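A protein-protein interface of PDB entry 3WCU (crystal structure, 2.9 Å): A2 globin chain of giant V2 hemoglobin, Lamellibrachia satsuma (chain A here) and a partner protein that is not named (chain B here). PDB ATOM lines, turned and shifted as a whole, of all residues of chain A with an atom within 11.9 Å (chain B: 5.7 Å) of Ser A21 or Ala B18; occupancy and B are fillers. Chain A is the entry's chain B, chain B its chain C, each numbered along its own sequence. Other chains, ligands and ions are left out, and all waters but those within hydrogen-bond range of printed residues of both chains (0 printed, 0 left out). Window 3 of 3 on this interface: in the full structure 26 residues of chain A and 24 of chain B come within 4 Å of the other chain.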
ATOM      1  N   LYS A  12      -0.024 -25.387  -1.358  1.00  0.00           N
ATOM      2  CA  LYS A  12      -0.626 -24.557  -2.392  1.00  0.00           C
ATOM      3  C   LYS A  12       0.484 -23.767  -3.071  1.00  0.00           C
ATOM      4  O   LYS A  12       0.599 -23.744  -4.301  1.00  0.00           O
ATOM      5  CB  LYS A  12      -1.623 -23.566  -1.788  1.00  0.00           C
ATOM      6  CG  LYS A  12      -2.829 -24.189  -1.131  1.00  0.00           C
ATOM      7  CD  LYS A  12      -3.699 -23.142  -0.449  1.00  0.00           C
ATOM      8  CE  LYS A  12      -4.429 -22.255  -1.454  1.00  0.00           C
ATOM      9  NZ  LYS A  12      -3.527 -21.325  -2.181  1.00  0.00           N
ATOM     10  N   ARG A  13       1.308 -23.122  -2.249  1.00  0.00           N
ATOM     11  CA  ARG A  13       2.391 -22.315  -2.760  1.00  0.00           C
ATOM     12  C   ARG A  13       3.413 -23.167  -3.475  1.00  0.00           C
ATOM     13  O   ARG A  13       3.519 -23.086  -4.695  1.00  0.00           O
ATOM     14  CB  ARG A  13       3.043 -21.536  -1.629  1.00  0.00           C
ATOM     15  CG  ARG A  13       4.073 -20.518  -2.088  1.00  0.00           C
ATOM     16  CD  ARG A  13       4.472 -19.595  -0.950  1.00  0.00           C
ATOM     17  NE  ARG A  13       4.800 -20.321   0.275  1.00  0.00           N
ATOM     18  CZ  ARG A  13       5.774 -21.221   0.384  1.00  0.00           C
ATOM     19  NH1 ARG A  13       5.984 -21.818   1.552  1.00  0.00           N
ATOM     20  NH2 ARG A  13       6.529 -21.525  -0.671  1.00  0.00           N
ATOM     21  N   GLN A  14       4.148 -24.001  -2.744  1.00  0.00           N
ATOM     22  CA  GLN A  14       5.167 -24.840  -3.379  1.00  0.00           C
ATOM     23  C   GLN A  14       4.737 -25.399  -4.743  1.00  0.00           C
ATOM     24  O   GLN A  14       5.554 -25.537  -5.656  1.00  0.00           O
ATOM     25  CB  GLN A  14       5.583 -25.995  -2.461  1.00  0.00           C
ATOM     26  CG  GLN A  14       6.037 -25.562  -1.079  1.00  0.00           C
ATOM     27  CD  GLN A  14       7.181 -26.393  -0.561  1.00  0.00           C
ATOM     28  OE1 GLN A  14       7.238 -27.597  -0.776  1.00  0.00           O
ATOM     29  NE2 GLN A  14       8.103 -25.750   0.136  1.00  0.00           N
ATOM     30  N   TRP A  15       3.453 -25.709  -4.890  1.00  0.00           N
ATOM     31  CA  TRP A  15       2.954 -26.249  -6.152  1.00  0.00           C
ATOM     32  C   TRP A  15       2.899 -25.171  -7.188  1.00  0.00           C
ATOM     33  O   TRP A  15       3.521 -25.290  -8.234  1.00  0.00           O
ATOM     34  CB  TRP A  15       1.550 -26.854  -5.980  1.00  0.00           C
ATOM     35  CG  TRP A  15       0.804 -27.049  -7.274  1.00  0.00           C
ATOM     36  CD1 TRP A  15      -0.142 -26.219  -7.806  1.00  0.00           C
ATOM     37  CD2 TRP A  15       0.960 -28.123  -8.201  1.00  0.00           C
ATOM     38  NE1 TRP A  15      -0.586 -26.711  -9.009  1.00  0.00           N
ATOM     39  CE2 TRP A  15       0.076 -27.882  -9.274  1.00  0.00           C
ATOM     40  CE3 TRP A  15       1.763 -29.269  -8.231  1.00  0.00           C
ATOM     41  CZ2 TRP A  15      -0.030 -28.747 -10.367  1.00  0.00           C
ATOM     42  CZ3 TRP A  15       1.660 -30.126  -9.318  1.00  0.00           C
ATOM     43  CH2 TRP A  15       0.769 -29.859 -10.370  1.00  0.00           C
ATOM     44  N   ALA A  16       2.133 -24.129  -6.877  1.00  0.00           N
ATOM     45  CA  ALA A  16       1.952 -22.988  -7.758  1.00  0.00           C
ATOM     46  C   ALA A  16       3.300 -22.530  -8.284  1.00  0.00           C
ATOM     47  O   ALA A  16       3.428 -22.191  -9.465  1.00  0.00           O
ATOM     48  CB  ALA A  16       1.274 -21.864  -7.009  1.00  0.00           C
ATOM     49  N   GLU A  17       4.301 -22.529  -7.403  1.00  0.00           N
ATOM     50  CA  GLU A  17       5.657 -22.136  -7.776  1.00  0.00           C
ATOM     51  C   GLU A  17       6.263 -23.109  -8.782  1.00  0.00           C
ATOM     52  O   GLU A  17       6.799 -22.698  -9.805  1.00  0.00           O
ATOM     53  CB  GLU A  17       6.569 -22.069  -6.548  1.00  0.00           C
ATOM     54  CG  GLU A  17       8.052 -22.111  -6.915  1.00  0.00           C
ATOM     55  CD  GLU A  17       8.970 -21.901  -5.734  1.00  0.00           C
ATOM     56  OE1 GLU A  17      10.202 -22.008  -5.904  1.00  0.00           O
ATOM     57  OE2 GLU A  17       8.455 -21.625  -4.631  1.00  0.00           O
ATOM     58  N   ALA A  18       6.180 -24.398  -8.481  1.00  0.00           N
ATOM     59  CA  ALA A  18       6.728 -25.414  -9.363  1.00  0.00           C
ATOM     60  C   ALA A  18       5.886 -25.650 -10.625  1.00  0.00           C
ATOM     61  O   ALA A  18       6.421 -26.002 -11.675  1.00  0.00           O
ATOM     62  CB  ALA A  18       6.915 -26.715  -8.588  1.00  0.00           C
ATOM     63  N   TYR A  19       4.574 -25.446 -10.538  1.00  0.00           N
ATOM     64  CA  TYR A  19       3.705 -25.652 -11.696  1.00  0.00           C
ATOM     65  C   TYR A  19       3.924 -24.513 -12.667  1.00  0.00           C
ATOM     66  O   TYR A  19       3.401 -24.505 -13.780  1.00  0.00           O
ATOM     67  CB  TYR A  19       2.237 -25.705 -11.253  1.00  0.00           C
ATOM     68  CG  TYR A  19       1.225 -25.937 -12.361  1.00  0.00           C
ATOM     69  CD1 TYR A  19       1.515 -26.753 -13.454  1.00  0.00           C
ATOM     70  CD2 TYR A  19      -0.049 -25.374 -12.284  1.00  0.00           C
ATOM     71  CE1 TYR A  19       0.556 -27.003 -14.444  1.00  0.00           C
ATOM     72  CE2 TYR A  19      -1.014 -25.619 -13.260  1.00  0.00           C
ATOM     73  CZ  TYR A  19      -0.710 -26.432 -14.337  1.00  0.00           C
ATOM     74  OH  TYR A  19      -1.679 -26.660 -15.295  1.00  0.00           O
ATOM     75  N   GLY A  20       4.716 -23.549 -12.224  1.00  0.00           N
ATOM     76  CA  GLY A  20       5.014 -22.405 -13.053  1.00  0.00           C
ATOM     77  C   GLY A  20       3.751 -21.720 -13.513  1.00  0.00           C
ATOM     78  O   GLY A  20       2.689 -21.854 -12.891  1.00  0.00           O
ATOM     79  N   SER A  21       3.873 -20.989 -14.614  1.00  0.00           N
ATOM     80  CA  SER A  21       2.744 -20.269 -15.160  1.00  0.00           C
ATOM     81  C   SER A  21       2.579 -20.437 -16.663  1.00  0.00           C
ATOM     82  O   SER A  21       1.716 -19.798 -17.273  1.00  0.00           O
ATOM     83  CB  SER A  21       2.855 -18.788 -14.826  1.00  0.00           C
ATOM     84  OG  SER A  21       1.729 -18.098 -15.331  1.00  0.00           O
ATOM     85  N   GLY A  22       3.404 -21.281 -17.271  1.00  0.00           N
ATOM     86  CA  GLY A  22       3.260 -21.496 -18.699  1.00  0.00           C
ATOM     87  C   GLY A  22       4.548 -21.521 -19.482  1.00  0.00           C
ATOM     88  O   GLY A  22       4.527 -21.481 -20.706  1.00  0.00           O
ATOM     89  N   ASN A  23       5.670 -21.582 -18.779  1.00  0.00           N
ATOM     90  CA  ASN A  23       6.970 -21.613 -19.433  1.00  0.00           C
ATOM     91  C   ASN A  23       7.609 -22.968 -19.193  1.00  0.00           C
ATOM     92  O   ASN A  23       7.708 -23.792 -20.104  1.00  0.00           O
ATOM     93  CB  ASN A  23       7.854 -20.498 -18.875  1.00  0.00           C
ATOM     94  CG  ASN A  23       7.280 -19.121 -19.139  1.00  0.00           C
ATOM     95  OD1 ASN A  23       7.698 -18.132 -18.533  1.00  0.00           O
ATOM     96  ND2 ASN A  23       6.318 -19.047 -20.056  1.00  0.00           N
ATOM     97  N   GLY A  24       8.032 -23.201 -17.958  1.00  0.00           N
ATOM     98  CA  GLY A  24       8.637 -24.475 -17.625  1.00  0.00           C
ATOM     99  C   GLY A  24       7.590 -25.539 -17.349  1.00  0.00           C
ATOM    100  O   GLY A  24       7.862 -26.525 -16.673  1.00  0.00           O
ATOM    101  N   ARG A  25       6.385 -25.340 -17.867  1.00  0.00           N
ATOM    102  CA  ARG A  25       5.317 -26.299 -17.661  1.00  0.00           C
ATOM    103  C   ARG A  25       5.532 -27.517 -18.532  1.00  0.00           C
ATOM    104  O   ARG A  25       5.541 -28.644 -18.039  1.00  0.00           O
ATOM    105  CB  ARG A  25       3.955 -25.680 -17.971  1.00  0.00           C
ATOM    106  CG  ARG A  25       3.111 -25.435 -16.734  1.00  0.00           C
ATOM    107  CD  ARG A  25       1.734 -25.000 -17.133  1.00  0.00           C
ATOM    108  NE  ARG A  25       1.011 -24.388 -16.031  1.00  0.00           N
ATOM    109  CZ  ARG A  25      -0.079 -23.646 -16.197  1.00  0.00           C
ATOM    110  NH1 ARG A  25      -0.556 -23.440 -17.423  1.00  0.00           N
ATOM    111  NH2 ARG A  25      -0.678 -23.090 -15.151  1.00  0.00           N
ATOM    112  N   GLU A  26       5.716 -27.301 -19.828  1.00  0.00           N
ATOM    113  CA  GLU A  26       5.936 -28.432 -20.704  1.00  0.00           C
ATOM    114  C   GLU A  26       7.073 -29.286 -20.149  1.00  0.00           C
ATOM    115  O   GLU A  26       7.137 -30.477 -20.417  1.00  0.00           O
ATOM    116  CB  GLU A  26       6.278 -27.988 -22.123  1.00  0.00           C
ATOM    117  CG  GLU A  26       5.986 -29.077 -23.143  1.00  0.00           C
ATOM    118  CD  GLU A  26       6.786 -28.935 -24.417  1.00  0.00           C
ATOM    119  OE1 GLU A  26       8.036 -28.971 -24.334  1.00  0.00           O
ATOM    120  OE2 GLU A  26       6.161 -28.796 -25.496  1.00  0.00           O
ATOM    121  N   GLU A  27       7.970 -28.685 -19.373  1.00  0.00           N
ATOM    122  CA  GLU A  27       9.071 -29.448 -18.797  1.00  0.00           C
ATOM    123  C   GLU A  27       8.589 -30.104 -17.505  1.00  0.00           C
ATOM    124  O   GLU A  27       8.931 -31.249 -17.224  1.00  0.00           O
ATOM    125  CB  GLU A  27      10.291 -28.550 -18.529  1.00  0.00           C
ATOM    126  CG  GLU A  27      11.570 -29.296 -18.124  1.00  0.00           C
ATOM    127  CD  GLU A  27      11.631 -29.638 -16.631  1.00  0.00           C
ATOM    128  OE1 GLU A  27      12.593 -30.328 -16.220  1.00  0.00           O
ATOM    129  OE2 GLU A  27      10.728 -29.216 -15.866  1.00  0.00           O
ATOM    130  N   PHE A  28       7.794 -29.390 -16.718  1.00  0.00           N
ATOM    131  CA  PHE A  28       7.281 -29.968 -15.486  1.00  0.00           C
ATOM    132  C   PHE A  28       6.641 -31.313 -15.849  1.00  0.00           C
ATOM    133  O   PHE A  28       7.074 -32.380 -15.391  1.00  0.00           O
ATOM    134  CB  PHE A  28       6.211 -29.068 -14.885  1.00  0.00           C
ATOM    135  CG  PHE A  28       5.844 -29.415 -13.462  1.00  0.00           C
ATOM    136  CD1 PHE A  28       4.582 -29.093 -12.962  1.00  0.00           C
ATOM    137  CD2 PHE A  28       6.785 -29.981 -12.599  1.00  0.00           C
ATOM    138  CE1 PHE A  28       4.270 -29.319 -11.631  1.00  0.00           C
ATOM    139  CE2 PHE A  28       6.485 -30.213 -11.265  1.00  0.00           C
ATOM    140  CZ  PHE A  28       5.225 -29.880 -10.774  1.00  0.00           C
ATOM    141  N   GLY A  29       5.607 -31.236 -16.684  1.00  0.00           N
ATOM    142  CA  GLY A  29       4.898 -32.416 -17.128  1.00  0.00           C
ATOM    143  C   GLY A  29       5.862 -33.480 -17.593  1.00  0.00           C
ATOM    144  O   GLY A  29       5.993 -34.517 -16.949  1.00  0.00           O
ATOM    145  N   THR A  65      -1.032 -32.117 -19.893  1.00  0.00           N
ATOM    146  CA  THR A  65      -1.477 -30.768 -19.574  1.00  0.00           C
ATOM    147  C   THR A  65      -2.848 -30.908 -18.895  1.00  0.00           C
ATOM    148  O   THR A  65      -3.121 -30.247 -17.886  1.00  0.00           O
ATOM    149  CB  THR A  65      -1.580 -29.864 -20.855  1.00  0.00           C
ATOM    150  OG1 THR A  65      -0.268 -29.571 -21.348  1.00  0.00           O
ATOM    151  CG2 THR A  65      -2.279 -28.546 -20.541  1.00  0.00           C
ATOM    152  N   LEU A  68      -2.177 -32.697 -15.066  1.00  0.00           N
ATOM    153  CA  LEU A  68      -1.582 -31.726 -14.145  1.00  0.00           C
ATOM    154  C   LEU A  68      -2.487 -30.514 -14.005  1.00  0.00           C
ATOM    155  O   LEU A  68      -2.497 -29.855 -12.966  1.00  0.00           O
ATOM    156  CB  LEU A  68      -0.195 -31.293 -14.629  1.00  0.00           C
ATOM    157  CG  LEU A  68       0.866 -32.382 -14.844  1.00  0.00           C
ATOM    158  CD1 LEU A  68       2.214 -31.710 -15.129  1.00  0.00           C
ATOM    159  CD2 LEU A  68       0.968 -33.288 -13.622  1.00  0.00           C
ATOM    160  N   GLY A  69      -3.248 -30.230 -15.055  1.00  0.00           N
ATOM    161  CA  GLY A  69      -4.177 -29.118 -15.005  1.00  0.00           C
ATOM    162  C   GLY A  69      -5.244 -29.416 -13.963  1.00  0.00           C
ATOM    163  O   GLY A  69      -5.756 -28.507 -13.294  1.00  0.00           O
ATOM    164  N   ASP A  72      -3.999 -29.320 -10.320  1.00  0.00           N
ATOM    165  CA  ASP A  72      -4.012 -27.941  -9.870  1.00  0.00           C
ATOM    166  C   ASP A  72      -5.366 -27.667  -9.240  1.00  0.00           C
ATOM    167  O   ASP A  72      -5.440 -27.354  -8.050  1.00  0.00           O
ATOM    168  CB  ASP A  72      -3.785 -26.979 -11.040  1.00  0.00           C
ATOM    169  CG  ASP A  72      -3.563 -25.543 -10.583  1.00  0.00           C
ATOM    170  OD1 ASP A  72      -3.888 -24.615 -11.348  1.00  0.00           O
ATOM    171  OD2 ASP A  72      -3.052 -25.346  -9.463  1.00  0.00           O
ATOM    172  N   GLU A 119      11.724 -29.013  -9.363  1.00  0.00           N
ATOM    173  CA  GLU A 119      11.509 -27.618  -9.715  1.00  0.00           C
ATOM    174  C   GLU A 119      11.943 -26.659  -8.600  1.00  0.00           C
ATOM    175  O   GLU A 119      12.774 -25.790  -8.828  1.00  0.00           O
ATOM    176  CB  GLU A 119      10.028 -27.404 -10.029  1.00  0.00           C
ATOM    177  CG  GLU A 119       9.703 -26.939 -11.436  1.00  0.00           C
ATOM    178  CD  GLU A 119      10.361 -27.762 -12.541  1.00  0.00           C
ATOM    179  OE1 GLU A 119      10.425 -29.009 -12.434  1.00  0.00           O
ATOM    180  OE2 GLU A 119      10.799 -27.147 -13.541  1.00  0.00           O
ATOM    181  N   ILE A 120      11.396 -26.828  -7.396  1.00  0.00           N
ATOM    182  CA  ILE A 120      11.701 -25.937  -6.272  1.00  0.00           C
ATOM    183  C   ILE A 120      12.875 -26.271  -5.358  1.00  0.00           C
ATOM    184  O   ILE A 120      13.137 -25.530  -4.411  1.00  0.00           O
ATOM    185  CB  ILE A 120      10.473 -25.723  -5.344  1.00  0.00           C
ATOM    186  CG1 ILE A 120      10.231 -26.960  -4.484  1.00  0.00           C
ATOM    187  CG2 ILE A 120       9.243 -25.411  -6.163  1.00  0.00           C
ATOM    188  CD1 ILE A 120       9.154 -26.744  -3.418  1.00  0.00           C
ATOM    189  N   MET B  13      -0.270 -11.428 -22.530  1.00  0.00           N
ATOM    190  CA  MET B  13      -1.410 -12.077 -21.902  1.00  0.00           C
ATOM    191  C   MET B  13      -0.931 -13.049 -20.814  1.00  0.00           C
ATOM    192  O   MET B  13      -1.448 -13.058 -19.689  1.00  0.00           O
ATOM    193  CB  MET B  13      -2.240 -12.853 -22.928  1.00  0.00           C
ATOM    194  CG  MET B  13      -3.336 -13.720 -22.294  1.00  0.00           C
ATOM    195  SD  MET B  13      -4.124 -14.874 -23.437  1.00  0.00           S
ATOM    196  CE  MET B  13      -5.830 -14.459 -23.185  1.00  0.00           C
ATOM    197  N   GLN B  14       0.062 -13.864 -21.155  1.00  0.00           N
ATOM    198  CA  GLN B  14       0.579 -14.854 -20.222  1.00  0.00           C
ATOM    199  C   GLN B  14       0.992 -14.229 -18.897  1.00  0.00           C
ATOM    200  O   GLN B  14       0.708 -14.770 -17.819  1.00  0.00           O
ATOM    201  CB  GLN B  14       1.761 -15.575 -20.850  1.00  0.00           C
ATOM    202  CG  GLN B  14       1.557 -17.044 -21.054  1.00  0.00           C
ATOM    203  CD  GLN B  14       2.506 -17.602 -22.099  1.00  0.00           C
ATOM    204  OE1 GLN B  14       2.709 -18.817 -22.186  1.00  0.00           O
ATOM    205  NE2 GLN B  14       3.089 -16.716 -22.909  1.00  0.00           N
ATOM    206  N   LEU B  15       1.656 -13.078 -18.988  1.00  0.00           N
ATOM    207  CA  LEU B  15       2.126 -12.358 -17.816  1.00  0.00           C
ATOM    208  C   LEU B  15       0.979 -11.790 -16.994  1.00  0.00           C
ATOM    209  O   LEU B  15       0.829 -12.111 -15.824  1.00  0.00           O
ATOM    210  CB  LEU B  15       3.050 -11.225 -18.245  1.00  0.00           C
ATOM    211  CG  LEU B  15       4.439 -11.317 -17.630  1.00  0.00           C
ATOM    212  CD1 LEU B  15       5.204 -10.091 -18.042  1.00  0.00           C
ATOM    213  CD2 LEU B  15       4.355 -11.427 -16.096  1.00  0.00           C
ATOM    214  N   MET B  16       0.174 -10.938 -17.616  1.00  0.00           N
ATOM    215  CA  MET B  16      -0.944 -10.337 -16.918  1.00  0.00           C
ATOM    216  C   MET B  16      -1.758 -11.414 -16.229  1.00  0.00           C
ATOM    217  O   MET B  16      -2.177 -11.241 -15.086  1.00  0.00           O
ATOM    218  CB  MET B  16      -1.814  -9.562 -17.902  1.00  0.00           C
ATOM    219  CG  MET B  16      -3.042  -8.942 -17.294  1.00  0.00           C
ATOM    220  SD  MET B  16      -4.503  -9.840 -17.801  1.00  0.00           S
ATOM    221  CE  MET B  16      -4.595 -11.083 -16.585  1.00  0.00           C
ATOM    222  N   TRP B  17      -1.975 -12.527 -16.927  1.00  0.00           N
ATOM    223  CA  TRP B  17      -2.753 -13.635 -16.394  1.00  0.00           C
ATOM    224  C   TRP B  17      -2.060 -14.282 -15.208  1.00  0.00           C
ATOM    225  O   TRP B  17      -2.626 -14.382 -14.122  1.00  0.00           O
ATOM    226  CB  TRP B  17      -3.021 -14.678 -17.494  1.00  0.00           C
ATOM    227  CG  TRP B  17      -3.929 -15.811 -17.066  1.00  0.00           C
ATOM    228  CD1 TRP B  17      -3.557 -17.073 -16.698  1.00  0.00           C
ATOM    229  CD2 TRP B  17      -5.342 -15.738 -16.859  1.00  0.00           C
ATOM    230  NE1 TRP B  17      -4.652 -17.789 -16.263  1.00  0.00           N
ATOM    231  CE2 TRP B  17      -5.758 -16.987 -16.351  1.00  0.00           C
ATOM    232  CE3 TRP B  17      -6.298 -14.730 -17.045  1.00  0.00           C
ATOM    233  CZ2 TRP B  17      -7.076 -17.253 -16.028  1.00  0.00           C
ATOM    234  CZ3 TRP B  17      -7.614 -14.995 -16.721  1.00  0.00           C
ATOM    235  CH2 TRP B  17      -7.990 -16.248 -16.217  1.00  0.00           C
ATOM    236  N   ALA B  18      -0.827 -14.715 -15.415  1.00  0.00           N
ATOM    237  CA  ALA B  18      -0.053 -15.363 -14.363  1.00  0.00           C
ATOM    238  C   ALA B  18      -0.181 -14.717 -12.971  1.00  0.00           C
ATOM    239  O   ALA B  18      -0.324 -15.413 -11.957  1.00  0.00           O
ATOM    240  CB  ALA B  18       1.414 -15.408 -14.778  1.00  0.00           C
ATOM    241  N   ASN B  19      -0.117 -13.391 -12.916  1.00  0.00           N
ATOM    242  CA  ASN B  19      -0.200 -12.711 -11.640  1.00  0.00           C
ATOM    243  C   ASN B  19      -1.547 -12.912 -10.969  1.00  0.00           C
ATOM    244  O   ASN B  19      -1.614 -13.298  -9.800  1.00  0.00           O
ATOM    245  CB  ASN B  19       0.103 -11.227 -11.807  1.00  0.00           C
ATOM    246  CG  ASN B  19       1.141 -10.750 -10.819  1.00  0.00           C
ATOM    247  OD1 ASN B  19       2.253 -11.297 -10.749  1.00  0.00           O
ATOM    248  ND2 ASN B  19       0.787  -9.731 -10.036  1.00  0.00           N
ATOM    249  N   VAL B  20      -2.621 -12.675 -11.709  1.00  0.00           N
ATOM    250  CA  VAL B  20      -3.956 -12.844 -11.149  1.00  0.00           C
ATOM    251  C   VAL B  20      -4.442 -14.268 -10.933  1.00  0.00           C
ATOM    252  O   VAL B  20      -5.251 -14.497 -10.047  1.00  0.00           O
ATOM    253  CB  VAL B  20      -5.024 -12.147 -11.995  1.00  0.00           C
ATOM    254  CG1 VAL B  20      -5.097 -10.690 -11.639  1.00  0.00           C
ATOM    255  CG2 VAL B  20      -4.719 -12.314 -13.450  1.00  0.00           C
ATOM    256  N   TRP B  21      -3.960 -15.229 -11.710  1.00  0.00           N
ATOM    257  CA  TRP B  21      -4.455 -16.604 -11.556  1.00  0.00           C
ATOM    258  C   TRP B  21      -3.439 -17.679 -11.175  1.00  0.00           C
ATOM    259  O   TRP B  21      -2.693 -18.182 -12.021  1.00  0.00           O
ATOM    260  CB  TRP B  21      -5.187 -17.009 -12.846  1.00  0.00           C
ATOM    261  CG  TRP B  21      -5.868 -18.346 -12.804  1.00  0.00           C
ATOM    262  CD1 TRP B  21      -5.292 -19.569 -13.001  1.00  0.00           C
ATOM    263  CD2 TRP B  21      -7.258 -18.594 -12.557  1.00  0.00           C
ATOM    264  NE1 TRP B  21      -6.238 -20.563 -12.894  1.00  0.00           N
ATOM    265  CE2 TRP B  21      -7.451 -19.990 -12.622  1.00  0.00           C
ATOM    266  CE3 TRP B  21      -8.357 -17.771 -12.283  1.00  0.00           C
ATOM    267  CZ2 TRP B  21      -8.697 -20.579 -12.425  1.00  0.00           C
ATOM    268  CZ3 TRP B  21      -9.591 -18.356 -12.086  1.00  0.00           C
ATOM    269  CH2 TRP B  21      -9.752 -19.747 -12.157  1.00  0.00           C
ATOM    270  N   SER B  22      -3.421 -18.056  -9.902  1.00  0.00           N
ATOM    271  CA  SER B  22      -2.478 -19.074  -9.456  1.00  0.00           C
ATOM    272  C   SER B  22      -2.939 -19.786  -8.196  1.00  0.00           C
ATOM    273  O   SER B  22      -3.646 -19.214  -7.370  1.00  0.00           O
ATOM    274  CB  SER B  22      -1.101 -18.452  -9.213  1.00  0.00           C
ATOM    275  OG  SER B  22      -1.157 -17.465  -8.199  1.00  0.00           O
ATOM    276  N   ASP B  76      -6.842 -21.295 -18.456  1.00  0.00           N
ATOM    277  CA  ASP B  76      -5.488 -21.209 -17.936  1.00  0.00           C
ATOM    278  C   ASP B  76      -4.594 -22.183 -18.670  1.00  0.00           C
ATOM    279  O   ASP B  76      -3.569 -21.800 -19.218  1.00  0.00           O
ATOM    280  CB  ASP B  76      -5.468 -21.512 -16.432  1.00  0.00           C
ATOM    281  CG  ASP B  76      -4.051 -21.645 -15.870  1.00  0.00           C
ATOM    282  OD1 ASP B  76      -3.801 -21.145 -14.757  1.00  0.00           O
ATOM    283  OD2 ASP B  76      -3.188 -22.261 -16.528  1.00  0.00           O
ATOM    284  N   GLY B  80      -1.419 -21.002 -21.058  1.00  0.00           N
ATOM    285  CA  GLY B  80      -0.084 -21.493 -20.789  1.00  0.00           C
ATOM    286  C   GLY B  80       0.447 -22.304 -21.953  1.00  0.00           C
ATOM    287  O   GLY B  80       1.659 -22.510 -22.088  1.00  0.00           O
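The guanidinium group (NH2) of Arg A25 is in salt-bridge range of the side-chain carboxylate (OD2) of Asp B76 (3.0 Å).
The backbone carbonyl oxygen (O) of Gly B80 lies close to the backbone carbonyl oxygen (O) of Gly A22, at 3.3 Å.
O of Tyr A19 sits close to NE of Arg A25 (3.3 Å).
NE1 of Trp B21 lies close to OD1 of Asp B76 (3.1 Å).
Ser A21 touches Ala B18 (OG to CB, 2.8 Å).
O of Gly A22 touches OE1 of Gln B14, at 3.5 Å.
Arg A25 touches Gly B80 (NH1 to CA, 3.9 Å).
Printed residues of chain B within 4 Å of Gly A22: Gln B14 (3.5 Å) and Gly B80 (3.3 Å).
Of the printed residues of chain B, Arg A25 touches Asp B76 and Gly B80.
Glu A27 touches none of the printed residues of chain B.
Of chain A, only Gly A22 (3.5 Å) comes within 4 Å of Gln B14.
No residue of chain A comes within 4 Å of Trp B17.
No residue of chain A comes within 4 Å of Asn B19.
No residue of chain A comes within 4 Å of Val B20.
No residue of chain A comes within 4 Å of Ser B22.
Of the printed residues of chain A, Asp B76 touches Arg A25 (3.0 Å).
Gly B80 touches two residues of chain A.
The nearest residue of chain A that does not touch Ala B18 is Gly A22 (6.7 Å).
Of the 12 printed residues of chain B, 4 touch a printed residue of chain A.
Hydrophobic or aromatic side chains of chain B that line the printed part of chain A: Ala B18.
Of the 24 printed residues of chain A, 3 touch a printed residue of chain B.
Along chain A the printed residues that touch a printed residue of chain B span positions 21 to 25.
Among the printed residues, Asp or Glu carboxylates within 4 Å of a Lys or Arg side-chain nitrogen of the other chain: Arg A25 with Asp B76 (3.0 Å).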
